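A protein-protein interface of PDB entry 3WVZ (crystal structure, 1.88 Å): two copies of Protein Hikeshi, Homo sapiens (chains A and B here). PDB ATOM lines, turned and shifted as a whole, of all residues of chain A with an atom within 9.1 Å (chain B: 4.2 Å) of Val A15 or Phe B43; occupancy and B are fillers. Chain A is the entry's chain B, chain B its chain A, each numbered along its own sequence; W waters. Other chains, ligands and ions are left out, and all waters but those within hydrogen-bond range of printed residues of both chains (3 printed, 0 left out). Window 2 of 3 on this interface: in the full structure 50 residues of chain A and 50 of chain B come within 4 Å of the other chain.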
ATOM      1  N   SER A   4      19.204  29.036 -21.829  1.00  0.00           N
ATOM      2  CA  SER A   4      17.795  29.406 -21.860  1.00  0.00           C
ATOM      3  C   SER A   4      16.969  28.414 -21.051  1.00  0.00           C
ATOM      4  O   SER A   4      17.331  27.244 -20.928  1.00  0.00           O
ATOM      5  CB  SER A   4      17.281  29.477 -23.300  1.00  0.00           C
ATOM      6  OG  SER A   4      17.849  30.575 -23.993  1.00  0.00           O
ATOM      7  N   PHE A   6      13.169  28.529 -21.118  1.00  0.00           N
ATOM      8  CA  PHE A   6      11.832  28.331 -21.669  1.00  0.00           C
ATOM      9  C   PHE A   6      11.782  28.237 -23.189  1.00  0.00           C
ATOM     10  O   PHE A   6      12.638  28.774 -23.891  1.00  0.00           O
ATOM     11  CB  PHE A   6      10.907  29.466 -21.228  1.00  0.00           C
ATOM     12  CG  PHE A   6      10.766  29.592 -19.738  1.00  0.00           C
ATOM     13  CD1 PHE A   6      10.010  28.677 -19.024  1.00  0.00           C
ATOM     14  CD2 PHE A   6      11.368  30.640 -19.056  1.00  0.00           C
ATOM     15  CE1 PHE A   6       9.868  28.794 -17.652  1.00  0.00           C
ATOM     16  CE2 PHE A   6      11.231  30.766 -17.684  1.00  0.00           C
ATOM     17  CZ  PHE A   6      10.479  29.841 -16.982  1.00  0.00           C
ATOM     18  N   GLY A   7      10.752  27.561 -23.685  1.00  0.00           N
ATOM     19  CA  GLY A   7      10.433  27.586 -25.098  1.00  0.00           C
ATOM     20  C   GLY A   7       9.061  28.204 -25.295  1.00  0.00           C
ATOM     21  O   GLY A   7       8.159  28.039 -24.464  1.00  0.00           O
ATOM     22  N   CYS A   8       8.904  28.928 -26.393  1.00  0.00           N
ATOM     23  CA  CYS A   8       7.624  29.518 -26.741  1.00  0.00           C
ATOM     24  C   CYS A   8       7.340  29.222 -28.202  1.00  0.00           C
ATOM     25  O   CYS A   8       8.107  29.606 -29.082  1.00  0.00           O
ATOM     26  CB  CYS A   8       7.629  31.026 -26.483  1.00  0.00           C
ATOM     27  SG  CYS A   8       6.034  31.818 -26.781  1.00  0.00           S
ATOM     28  N   LEU A   9       6.241  28.526 -28.456  1.00  0.00           N
ATOM     29  CA  LEU A   9       5.944  28.065 -29.800  1.00  0.00           C
ATOM     30  C   LEU A   9       4.571  28.537 -30.273  1.00  0.00           C
ATOM     31  O   LEU A   9       3.549  28.172 -29.693  1.00  0.00           O
ATOM     32  CB  LEU A   9       6.027  26.538 -29.843  1.00  0.00           C
ATOM     33  CG  LEU A   9       5.634  25.825 -31.134  1.00  0.00           C
ATOM     34  CD1 LEU A   9       6.491  26.310 -32.274  1.00  0.00           C
ATOM     35  CD2 LEU A   9       5.793  24.327 -30.949  1.00  0.00           C
ATOM     36  N   VAL A  10       4.565  29.367 -31.311  1.00  0.00           N
ATOM     37  CA  VAL A  10       3.336  29.693 -32.023  1.00  0.00           C
ATOM     38  C   VAL A  10       3.086  28.593 -33.046  1.00  0.00           C
ATOM     39  O   VAL A  10       3.941  28.325 -33.890  1.00  0.00           O
ATOM     40  CB  VAL A  10       3.414  31.057 -32.734  1.00  0.00           C
ATOM     41  CG1 VAL A  10       2.184  31.258 -33.610  1.00  0.00           C
ATOM     42  CG2 VAL A  10       3.560  32.194 -31.715  1.00  0.00           C
ATOM     43  N   ALA A  11       1.922  27.958 -32.966  1.00  0.00           N
ATOM     44  CA  ALA A  11       1.579  26.894 -33.900  1.00  0.00           C
ATOM     45  C   ALA A  11       1.713  27.406 -35.329  1.00  0.00           C
ATOM     46  O   ALA A  11       1.147  28.439 -35.689  1.00  0.00           O
ATOM     47  CB  ALA A  11       0.172  26.374 -33.638  1.00  0.00           C
ATOM     48  N   GLY A  12       2.502  26.693 -36.128  1.00  0.00           N
ATOM     49  CA  GLY A  12       2.761  27.080 -37.503  1.00  0.00           C
ATOM     50  C   GLY A  12       4.133  27.703 -37.673  1.00  0.00           C
ATOM     51  O   GLY A  12       4.570  27.964 -38.795  1.00  0.00           O
ATOM     52  N   ARG A  13       4.809  27.955 -36.551  1.00  0.00           N
ATOM     53  CA  ARG A  13       6.152  28.532 -36.570  1.00  0.00           C
ATOM     54  C   ARG A  13       7.145  27.644 -35.817  1.00  0.00           C
ATOM     55  O   ARG A  13       6.795  26.554 -35.373  1.00  0.00           O
ATOM     56  CB  ARG A  13       6.141  29.935 -35.953  1.00  0.00           C
ATOM     57  CG  ARG A  13       5.057  30.834 -36.512  1.00  0.00           C
ATOM     58  CD  ARG A  13       5.101  32.215 -35.874  1.00  0.00           C
ATOM     59  NE  ARG A  13       3.942  33.020 -36.241  1.00  0.00           N
ATOM     60  CZ  ARG A  13       3.682  34.220 -35.729  1.00  0.00           C
ATOM     61  NH1 ARG A  13       4.497  34.743 -34.825  1.00  0.00           N
ATOM     62  NH2 ARG A  13       2.603  34.889 -36.110  1.00  0.00           N
ATOM     63  N   LEU A  14       8.385  28.109 -35.687  1.00  0.00           N
ATOM     64  CA  LEU A  14       9.402  27.371 -34.933  1.00  0.00           C
ATOM     65  C   LEU A  14       9.418  27.775 -33.470  1.00  0.00           C
ATOM     66  O   LEU A  14       8.902  28.829 -33.108  1.00  0.00           O
ATOM     67  CB  LEU A  14      10.786  27.600 -35.528  1.00  0.00           C
ATOM     68  CG  LEU A  14      11.053  26.967 -36.890  1.00  0.00           C
ATOM     69  CD1 LEU A  14      12.273  27.607 -37.472  1.00  0.00           C
ATOM     70  CD2 LEU A  14      11.249  25.457 -36.770  1.00  0.00           C
ATOM     71  N   VAL A  15      10.034  26.946 -32.633  1.00  0.00           N
ATOM     72  CA  VAL A  15      10.170  27.274 -31.218  1.00  0.00           C
ATOM     73  C   VAL A  15      11.107  28.454 -31.037  1.00  0.00           C
ATOM     74  O   VAL A  15      12.180  28.502 -31.639  1.00  0.00           O
ATOM     75  CB  VAL A  15      10.704  26.079 -30.397  1.00  0.00           C
ATOM     76  CG1 VAL A  15      10.869  26.470 -28.929  1.00  0.00           C
ATOM     77  CG2 VAL A  15       9.775  24.888 -30.525  1.00  0.00           C
ATOM     78  N   GLN A  16      10.686  29.415 -30.223  1.00  0.00           N
ATOM     79  CA  GLN A  16      11.557  30.506 -29.808  1.00  0.00           C
ATOM     80  C   GLN A  16      12.110  30.181 -28.424  1.00  0.00           C
ATOM     81  O   GLN A  16      11.355  29.808 -27.529  1.00  0.00           O
ATOM     82  CB  GLN A  16      10.801  31.840 -29.781  1.00  0.00           C
ATOM     83  CG  GLN A  16      10.314  32.342 -31.141  1.00  0.00           C
ATOM     84  CD  GLN A  16       9.559  33.661 -31.024  1.00  0.00           C
ATOM     85  OE1 GLN A  16       8.996  33.969 -29.976  1.00  0.00           O
ATOM     86  NE2 GLN A  16       9.564  34.453 -32.094  1.00  0.00           N
ATOM     87  N   THR A  17      13.419  30.315 -28.238  1.00  0.00           N
ATOM     88  CA  THR A  17      14.020  29.993 -26.939  1.00  0.00           C
ATOM     89  C   THR A  17      14.792  31.164 -26.350  1.00  0.00           C
ATOM     90  O   THR A  17      15.045  31.209 -25.144  1.00  0.00           O
ATOM     91  CB  THR A  17      14.977  28.793 -27.034  1.00  0.00           C
ATOM     92  OG1 THR A  17      16.027  29.089 -27.967  1.00  0.00           O
ATOM     93  CG2 THR A  17      14.232  27.544 -27.485  1.00  0.00           C
ATOM     94  N   ALA A  18      15.174  32.105 -27.202  1.00  0.00           N
ATOM     95  CA  ALA A  18      15.988  33.229 -26.762  1.00  0.00           C
ATOM     96  C   ALA A  18      15.102  34.353 -26.238  1.00  0.00           C
ATOM     97  O   ALA A  18      14.902  35.363 -26.907  1.00  0.00           O
ATOM     98  CB  ALA A  18      16.872  33.721 -27.900  1.00  0.00           C
ATOM     99  N   ALA A  19      14.569  34.161 -25.036  1.00  0.00           N
ATOM    100  CA  ALA A  19      13.691  35.145 -24.419  1.00  0.00           C
ATOM    101  C   ALA A  19      14.477  36.372 -23.987  1.00  0.00           C
ATOM    102  O   ALA A  19      15.654  36.273 -23.650  1.00  0.00           O
ATOM    103  CB  ALA A  19      12.973  34.546 -23.232  1.00  0.00           C
ATOM    104  N   PHE A  29       8.786  36.957 -24.599  1.00  0.00           N
ATOM    105  CA  PHE A  29       8.946  36.630 -26.011  1.00  0.00           C
ATOM    106  C   PHE A  29       8.122  37.578 -26.877  1.00  0.00           C
ATOM    107  O   PHE A  29       6.916  37.709 -26.669  1.00  0.00           O
ATOM    108  CB  PHE A  29       8.500  35.192 -26.308  1.00  0.00           C
ATOM    109  CG  PHE A  29       9.341  34.132 -25.653  1.00  0.00           C
ATOM    110  CD1 PHE A  29      10.434  33.590 -26.312  1.00  0.00           C
ATOM    111  CD2 PHE A  29       9.018  33.654 -24.399  1.00  0.00           C
ATOM    112  CE1 PHE A  29      11.206  32.604 -25.716  1.00  0.00           C
ATOM    113  CE2 PHE A  29       9.782  32.667 -23.795  1.00  0.00           C
ATOM    114  CZ  PHE A  29      10.873  32.138 -24.461  1.00  0.00           C
ATOM    115  N   LEU A  31       6.242  38.197 -30.300  1.00  0.00           N
ATOM    116  CA  LEU A  31       5.642  37.370 -31.342  1.00  0.00           C
ATOM    117  C   LEU A  31       5.127  38.234 -32.491  1.00  0.00           C
ATOM    118  O   LEU A  31       4.153  38.964 -32.324  1.00  0.00           O
ATOM    119  CB  LEU A  31       4.501  36.533 -30.765  1.00  0.00           C
ATOM    120  CG  LEU A  31       4.824  35.745 -29.492  1.00  0.00           C
ATOM    121  CD1 LEU A  31       3.571  35.083 -28.956  1.00  0.00           C
ATOM    122  CD2 LEU A  31       5.893  34.712 -29.779  1.00  0.00           C
ATOM    123  N   VAL A  41       2.250  27.547 -27.509  1.00  0.00           N
ATOM    124  CA  VAL A  41       2.678  26.507 -26.594  1.00  0.00           C
ATOM    125  C   VAL A  41       3.869  27.038 -25.807  1.00  0.00           C
ATOM    126  O   VAL A  41       4.839  27.522 -26.396  1.00  0.00           O
ATOM    127  CB  VAL A  41       3.057  25.205 -27.340  1.00  0.00           C
ATOM    128  CG1 VAL A  41       3.358  24.097 -26.353  1.00  0.00           C
ATOM    129  CG2 VAL A  41       1.927  24.784 -28.278  1.00  0.00           C
ATOM    130  N   VAL A  42       3.773  26.980 -24.483  1.00  0.00           N
ATOM    131  CA  VAL A  42       4.820  27.490 -23.600  1.00  0.00           C
ATOM    132  C   VAL A  42       5.341  26.336 -22.756  1.00  0.00           C
ATOM    133  O   VAL A  42       4.556  25.577 -22.184  1.00  0.00           O
ATOM    134  CB  VAL A  42       4.306  28.621 -22.684  1.00  0.00           C
ATOM    135  CG1 VAL A  42       5.424  29.143 -21.796  1.00  0.00           C
ATOM    136  CG2 VAL A  42       3.691  29.752 -23.509  1.00  0.00           C
ATOM    137  N   PHE A  43       6.657  26.180 -22.674  1.00  0.00           N
ATOM    138  CA  PHE A  43       7.175  25.000 -22.000  1.00  0.00           C
ATOM    139  C   PHE A  43       8.591  25.185 -21.456  1.00  0.00           C
ATOM    140  O   PHE A  43       9.337  26.063 -21.899  1.00  0.00           O
ATOM    141  CB  PHE A  43       7.115  23.791 -22.947  1.00  0.00           C
ATOM    142  CG  PHE A  43       7.883  23.974 -24.230  1.00  0.00           C
ATOM    143  CD1 PHE A  43       7.281  24.555 -25.338  1.00  0.00           C
ATOM    144  CD2 PHE A  43       9.198  23.549 -24.333  1.00  0.00           C
ATOM    145  CE1 PHE A  43       7.982  24.719 -26.519  1.00  0.00           C
ATOM    146  CE2 PHE A  43       9.906  23.707 -25.513  1.00  0.00           C
ATOM    147  CZ  PHE A  43       9.296  24.293 -26.608  1.00  0.00           C
ATOM    148  N   MET A  44       8.935  24.370 -20.466  1.00  0.00           N
ATOM    149  CA  MET A  44      10.296  24.328 -19.945  1.00  0.00           C
ATOM    150  C   MET A  44      11.161  23.484 -20.868  1.00  0.00           C
ATOM    151  O   MET A  44      10.730  22.432 -21.336  1.00  0.00           O
ATOM    152  CB  MET A  44      10.324  23.754 -18.527  1.00  0.00           C
ATOM    153  CG  MET A  44       9.393  24.447 -17.536  1.00  0.00           C
ATOM    154  SD  MET A  44       9.575  23.766 -15.871  1.00  0.00           S
ATOM    155  CE  MET A  44      11.182  24.423 -15.404  1.00  0.00           C
ATOM    156  N   LEU A  45      12.390  23.927 -21.107  1.00  0.00           N
ATOM    157  CA  LEU A  45      13.295  23.204 -21.995  1.00  0.00           C
ATOM    158  C   LEU A  45      13.877  21.958 -21.322  1.00  0.00           C
ATOM    159  O   LEU A  45      14.391  21.067 -21.992  1.00  0.00           O
ATOM    160  CB  LEU A  45      14.424  24.122 -22.467  1.00  0.00           C
ATOM    161  CG  LEU A  45      14.008  25.389 -23.226  1.00  0.00           C
ATOM    162  CD1 LEU A  45      15.239  26.157 -23.686  1.00  0.00           C
ATOM    163  CD2 LEU A  45      13.111  25.045 -24.408  1.00  0.00           C
ATOM    164  N   PHE B   6      13.230  16.472 -35.257  1.00  0.00           N
ATOM    165  CA  PHE B   6      11.872  16.789 -34.813  1.00  0.00           C
ATOM    166  C   PHE B   6      11.713  16.754 -33.303  1.00  0.00           C
ATOM    167  O   PHE B   6      12.452  16.065 -32.600  1.00  0.00           O
ATOM    168  CB  PHE B   6      10.866  15.824 -35.432  1.00  0.00           C
ATOM    169  CG  PHE B   6      10.848  15.844 -36.927  1.00  0.00           C
ATOM    170  CD1 PHE B   6      10.171  16.842 -37.612  1.00  0.00           C
ATOM    171  CD2 PHE B   6      11.504  14.863 -37.651  1.00  0.00           C
ATOM    172  CE1 PHE B   6      10.152  16.860 -38.999  1.00  0.00           C
ATOM    173  CE2 PHE B   6      11.488  14.873 -39.035  1.00  0.00           C
ATOM    174  CZ  PHE B   6      10.813  15.875 -39.710  1.00  0.00           C
ATOM    175  N   GLY B   7      10.721  17.492 -32.825  1.00  0.00           N
ATOM    176  CA  GLY B   7      10.333  17.463 -31.430  1.00  0.00           C
ATOM    177  C   GLY B   7       8.872  17.083 -31.295  1.00  0.00           C
ATOM    178  O   GLY B   7       8.079  17.261 -32.224  1.00  0.00           O
ATOM    179  N   CYS B   8       8.518  16.569 -30.124  1.00  0.00           N
ATOM    180  CA  CYS B   8       7.163  16.119 -29.843  1.00  0.00           C
ATOM    181  C   CYS B   8       6.790  16.555 -28.431  1.00  0.00           C
ATOM    182  O   CYS B   8       7.582  16.396 -27.504  1.00  0.00           O
ATOM    183  CB  CYS B   8       7.075  14.597 -29.994  1.00  0.00           C
ATOM    184  SG  CYS B   8       5.469  13.881 -29.625  1.00  0.00           S
ATOM    185  N   VAL B  15       9.053  18.222 -23.384  1.00  0.00           N
ATOM    186  CA  VAL B  15       9.331  17.998 -24.799  1.00  0.00           C
ATOM    187  C   VAL B  15      10.222  16.775 -25.009  1.00  0.00           C
ATOM    188  O   VAL B  15      11.199  16.577 -24.284  1.00  0.00           O
ATOM    189  CB  VAL B  15      10.005  19.232 -25.447  1.00  0.00           C
ATOM    190  CG1 VAL B  15      10.621  18.879 -26.793  1.00  0.00           C
ATOM    191  CG2 VAL B  15       9.003  20.339 -25.618  1.00  0.00           C
ATOM    192  N   VAL B  41       1.682  18.068 -29.864  1.00  0.00           N
ATOM    193  CA  VAL B  41       2.353  19.098 -30.645  1.00  0.00           C
ATOM    194  C   VAL B  41       3.573  18.487 -31.333  1.00  0.00           C
ATOM    195  O   VAL B  41       4.397  17.850 -30.678  1.00  0.00           O
ATOM    196  CB  VAL B  41       2.799  20.288 -29.752  1.00  0.00           C
ATOM    197  CG1 VAL B  41       3.318  21.433 -30.599  1.00  0.00           C
ATOM    198  CG2 VAL B  41       1.655  20.753 -28.858  1.00  0.00           C
ATOM    199  N   VAL B  42       3.687  18.667 -32.645  1.00  0.00           N
ATOM    200  CA  VAL B  42       4.830  18.151 -33.395  1.00  0.00           C
ATOM    201  C   VAL B  42       5.513  19.297 -34.124  1.00  0.00           C
ATOM    202  O   VAL B  42       4.841  20.139 -34.717  1.00  0.00           O
ATOM    203  CB  VAL B  42       4.404  17.066 -34.412  1.00  0.00           C
ATOM    204  CG1 VAL B  42       5.595  16.597 -35.237  1.00  0.00           C
ATOM    205  CG2 VAL B  42       3.751  15.899 -33.694  1.00  0.00           C
ATOM    206  N   PHE B  43       6.840  19.344 -34.081  1.00  0.00           N
ATOM    207  CA  PHE B  43       7.552  20.473 -34.671  1.00  0.00           C
ATOM    208  C   PHE B  43       8.966  20.142 -35.128  1.00  0.00           C
ATOM    209  O   PHE B  43       9.632  19.284 -34.556  1.00  0.00           O
ATOM    210  CB  PHE B  43       7.595  21.651 -33.683  1.00  0.00           C
ATOM    211  CG  PHE B  43       8.167  21.306 -32.332  1.00  0.00           C
ATOM    212  CD1 PHE B  43       7.359  20.784 -31.335  1.00  0.00           C
ATOM    213  CD2 PHE B  43       9.507  21.538 -32.050  1.00  0.00           C
ATOM    214  CE1 PHE B  43       7.878  20.472 -30.089  1.00  0.00           C
ATOM    215  CE2 PHE B  43      10.036  21.228 -30.798  1.00  0.00           C
ATOM    216  CZ  PHE B  43       9.220  20.699 -29.819  1.00  0.00           C
ATOM    217  N   MET B  44       9.411  20.827 -36.179  1.00  0.00           N
ATOM    218  CA  MET B  44      10.820  20.814 -36.551  1.00  0.00           C
ATOM    219  C   MET B  44      11.628  21.501 -35.454  1.00  0.00           C
ATOM    220  O   MET B  44      11.179  22.497 -34.877  1.00  0.00           O
ATOM    221  CB  MET B  44      11.055  21.526 -37.885  1.00  0.00           C
ATOM    222  CG  MET B  44      10.243  20.996 -39.056  1.00  0.00           C
ATOM    223  SD  MET B  44      10.611  21.909 -40.568  1.00  0.00           S
ATOM    224  CE  MET B  44      12.326  21.475 -40.844  1.00  0.00           C
ATOM    225  N   LEU B  45      12.818  20.982 -35.172  1.00  0.00           N
ATOM    226  CA  LEU B  45      13.684  21.593 -34.171  1.00  0.00           C
ATOM    227  C   LEU B  45      14.363  22.850 -34.705  1.00  0.00           C
ATOM    228  O   LEU B  45      14.847  23.678 -33.937  1.00  0.00           O
ATOM    229  CB  LEU B  45      14.739  20.589 -33.690  1.00  0.00           C
ATOM    230  CG  LEU B  45      14.198  19.328 -33.016  1.00  0.00           C
ATOM    231  CD1 LEU B  45      15.342  18.412 -32.609  1.00  0.00           C
ATOM    232  CD2 LEU B  45      13.338  19.685 -31.807  1.00  0.00           C
ATOM    233  N   PRO B  82       6.364  24.721 -39.983  1.00  0.00           N
ATOM    234  CA  PRO B  82       7.202  23.713 -39.320  1.00  0.00           C
ATOM    235  C   PRO B  82       6.662  23.139 -38.012  1.00  0.00           C
ATOM    236  O   PRO B  82       7.372  22.353 -37.383  1.00  0.00           O
ATOM    237  CB  PRO B  82       8.508  24.474 -39.062  1.00  0.00           C
ATOM    238  CG  PRO B  82       8.083  25.897 -38.926  1.00  0.00           C
ATOM    239  CD  PRO B  82       6.942  26.073 -39.885  1.00  0.00           C
ATOM    240  N   SER B  83       5.452  23.510 -37.610  1.00  0.00           N
ATOM    241  CA  SER B  83       4.849  22.934 -36.414  1.00  0.00           C
ATOM    242  C   SER B  83       3.332  22.855 -36.532  1.00  0.00           C
ATOM    243  O   SER B  83       2.711  23.618 -37.278  1.00  0.00           O
ATOM    244  CB  SER B  83       5.224  23.753 -35.175  1.00  0.00           C
ATOM    245  OG  SER B  83       4.689  25.064 -35.258  1.00  0.00           O
HETATM  246  O   HOH W   1       8.564  20.708 -21.192  1.00  0.00           O
HETATM  247  O   HOH W   2      11.650  24.663 -33.328  1.00  0.00           O
HETATM  248  O   HOH W   3      13.938  26.714 -33.010  1.00  0.00           O
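The side-chain hydroxyl of Ser B83 lies within hydrogen-bond range of the backbone NH of Gly A12 (2.9 Å). The side-chain hydroxyl (OG) of Ser B83 lies within hydrogen-bond range of the backbone carbonyl oxygen (O) of Arg A13, at 2.6 Å.
The backbone NH of Gly B7 lies within hydrogen-bond range of the backbone carbonyl oxygen of Phe B43 (2.7 Å). The backbone NH (N) of Met B44 is in hydrogen-bond range of the backbone carbonyl oxygen (O) of Pro B82, at 2.8 Å. N of Gly A7 lies within hydrogen-bond range of O of Phe A43, 2.7 Å away. O of Leu A9 is in hydrogen-bond range of N of Val A41 (2.6 Å).
Among the printed residues, pairs that only touch across the chains: Leu A9 with Val B41, Leu A9 with Phe B43, Leu A9 with Ser B83, Val A10 with Ser B83, Ala A11 with Ser B83, Gly A12 with Pro B82, Arg A13 with Pro B82, Leu A14 with Met B44, Leu A14 with Pro B82, Val A15 with Phe B43 and Phe A43 with Val B15.
Printed residues of chain B within 4 Å of Gly A12: Pro B82 (3.2 Å) and Ser B83 (2.9 Å). Printed residues of chain B within 4 Å of Leu A14: Met B44 (3.5 Å) and Pro B82 (3.7 Å). Val A15 touches just one residue of chain B: Phe B43. Thr A17 touches none of the printed residues of chain B. Printed residues of chain A within 4 Å of Val B15: Phe A43. No residue of chain A comes within 4 Å of Val B42. Phe B43 touches two residues of chain A. Of the printed residues of chain A, Pro B82 touches Gly A12, Arg A13 and Leu A14. The nearest printed residue of chain B that does not touch Val A15 is Met B44 (5.1 Å).
Hydrophobic or aromatic side chains of chain A that line the printed part of chain B: Leu A9, Leu A14, Val A15 and Phe A43. Hydrophobic or aromatic side chains of chain B that line the printed part of chain A: Val B15, Val B41, Phe B43 and Pro B82. Among the printed residues, no Asp or Glu carboxylate lies within 4 Å of a Lys or Arg side-chain nitrogen of the other chain.
Val A15 touches Phe B43, and with the chains exchanged Phe A43 touches Val B15. Positions printed for both chains: 6, 7, 8, 15, 41, 42, 43, 44 and 45. Of the 13 pairs that touch across the chains among the printed residues, 2 have their exchanged pair printed and touching as well.
Water W2 lies within hydrogen-bond range of the backbone carbonyl oxygen (O) of Met B44, the backbone NH (N) of Val A15 and the backbone carbonyl oxygen (O) of Leu B45. Water W1 bridges O of Met A44 (2.8 Å) and N of Val B15 (3.4 Å). Water W3 bridges O of Val A15 (2.9 Å) and O of Leu B45 (3.3 Å).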
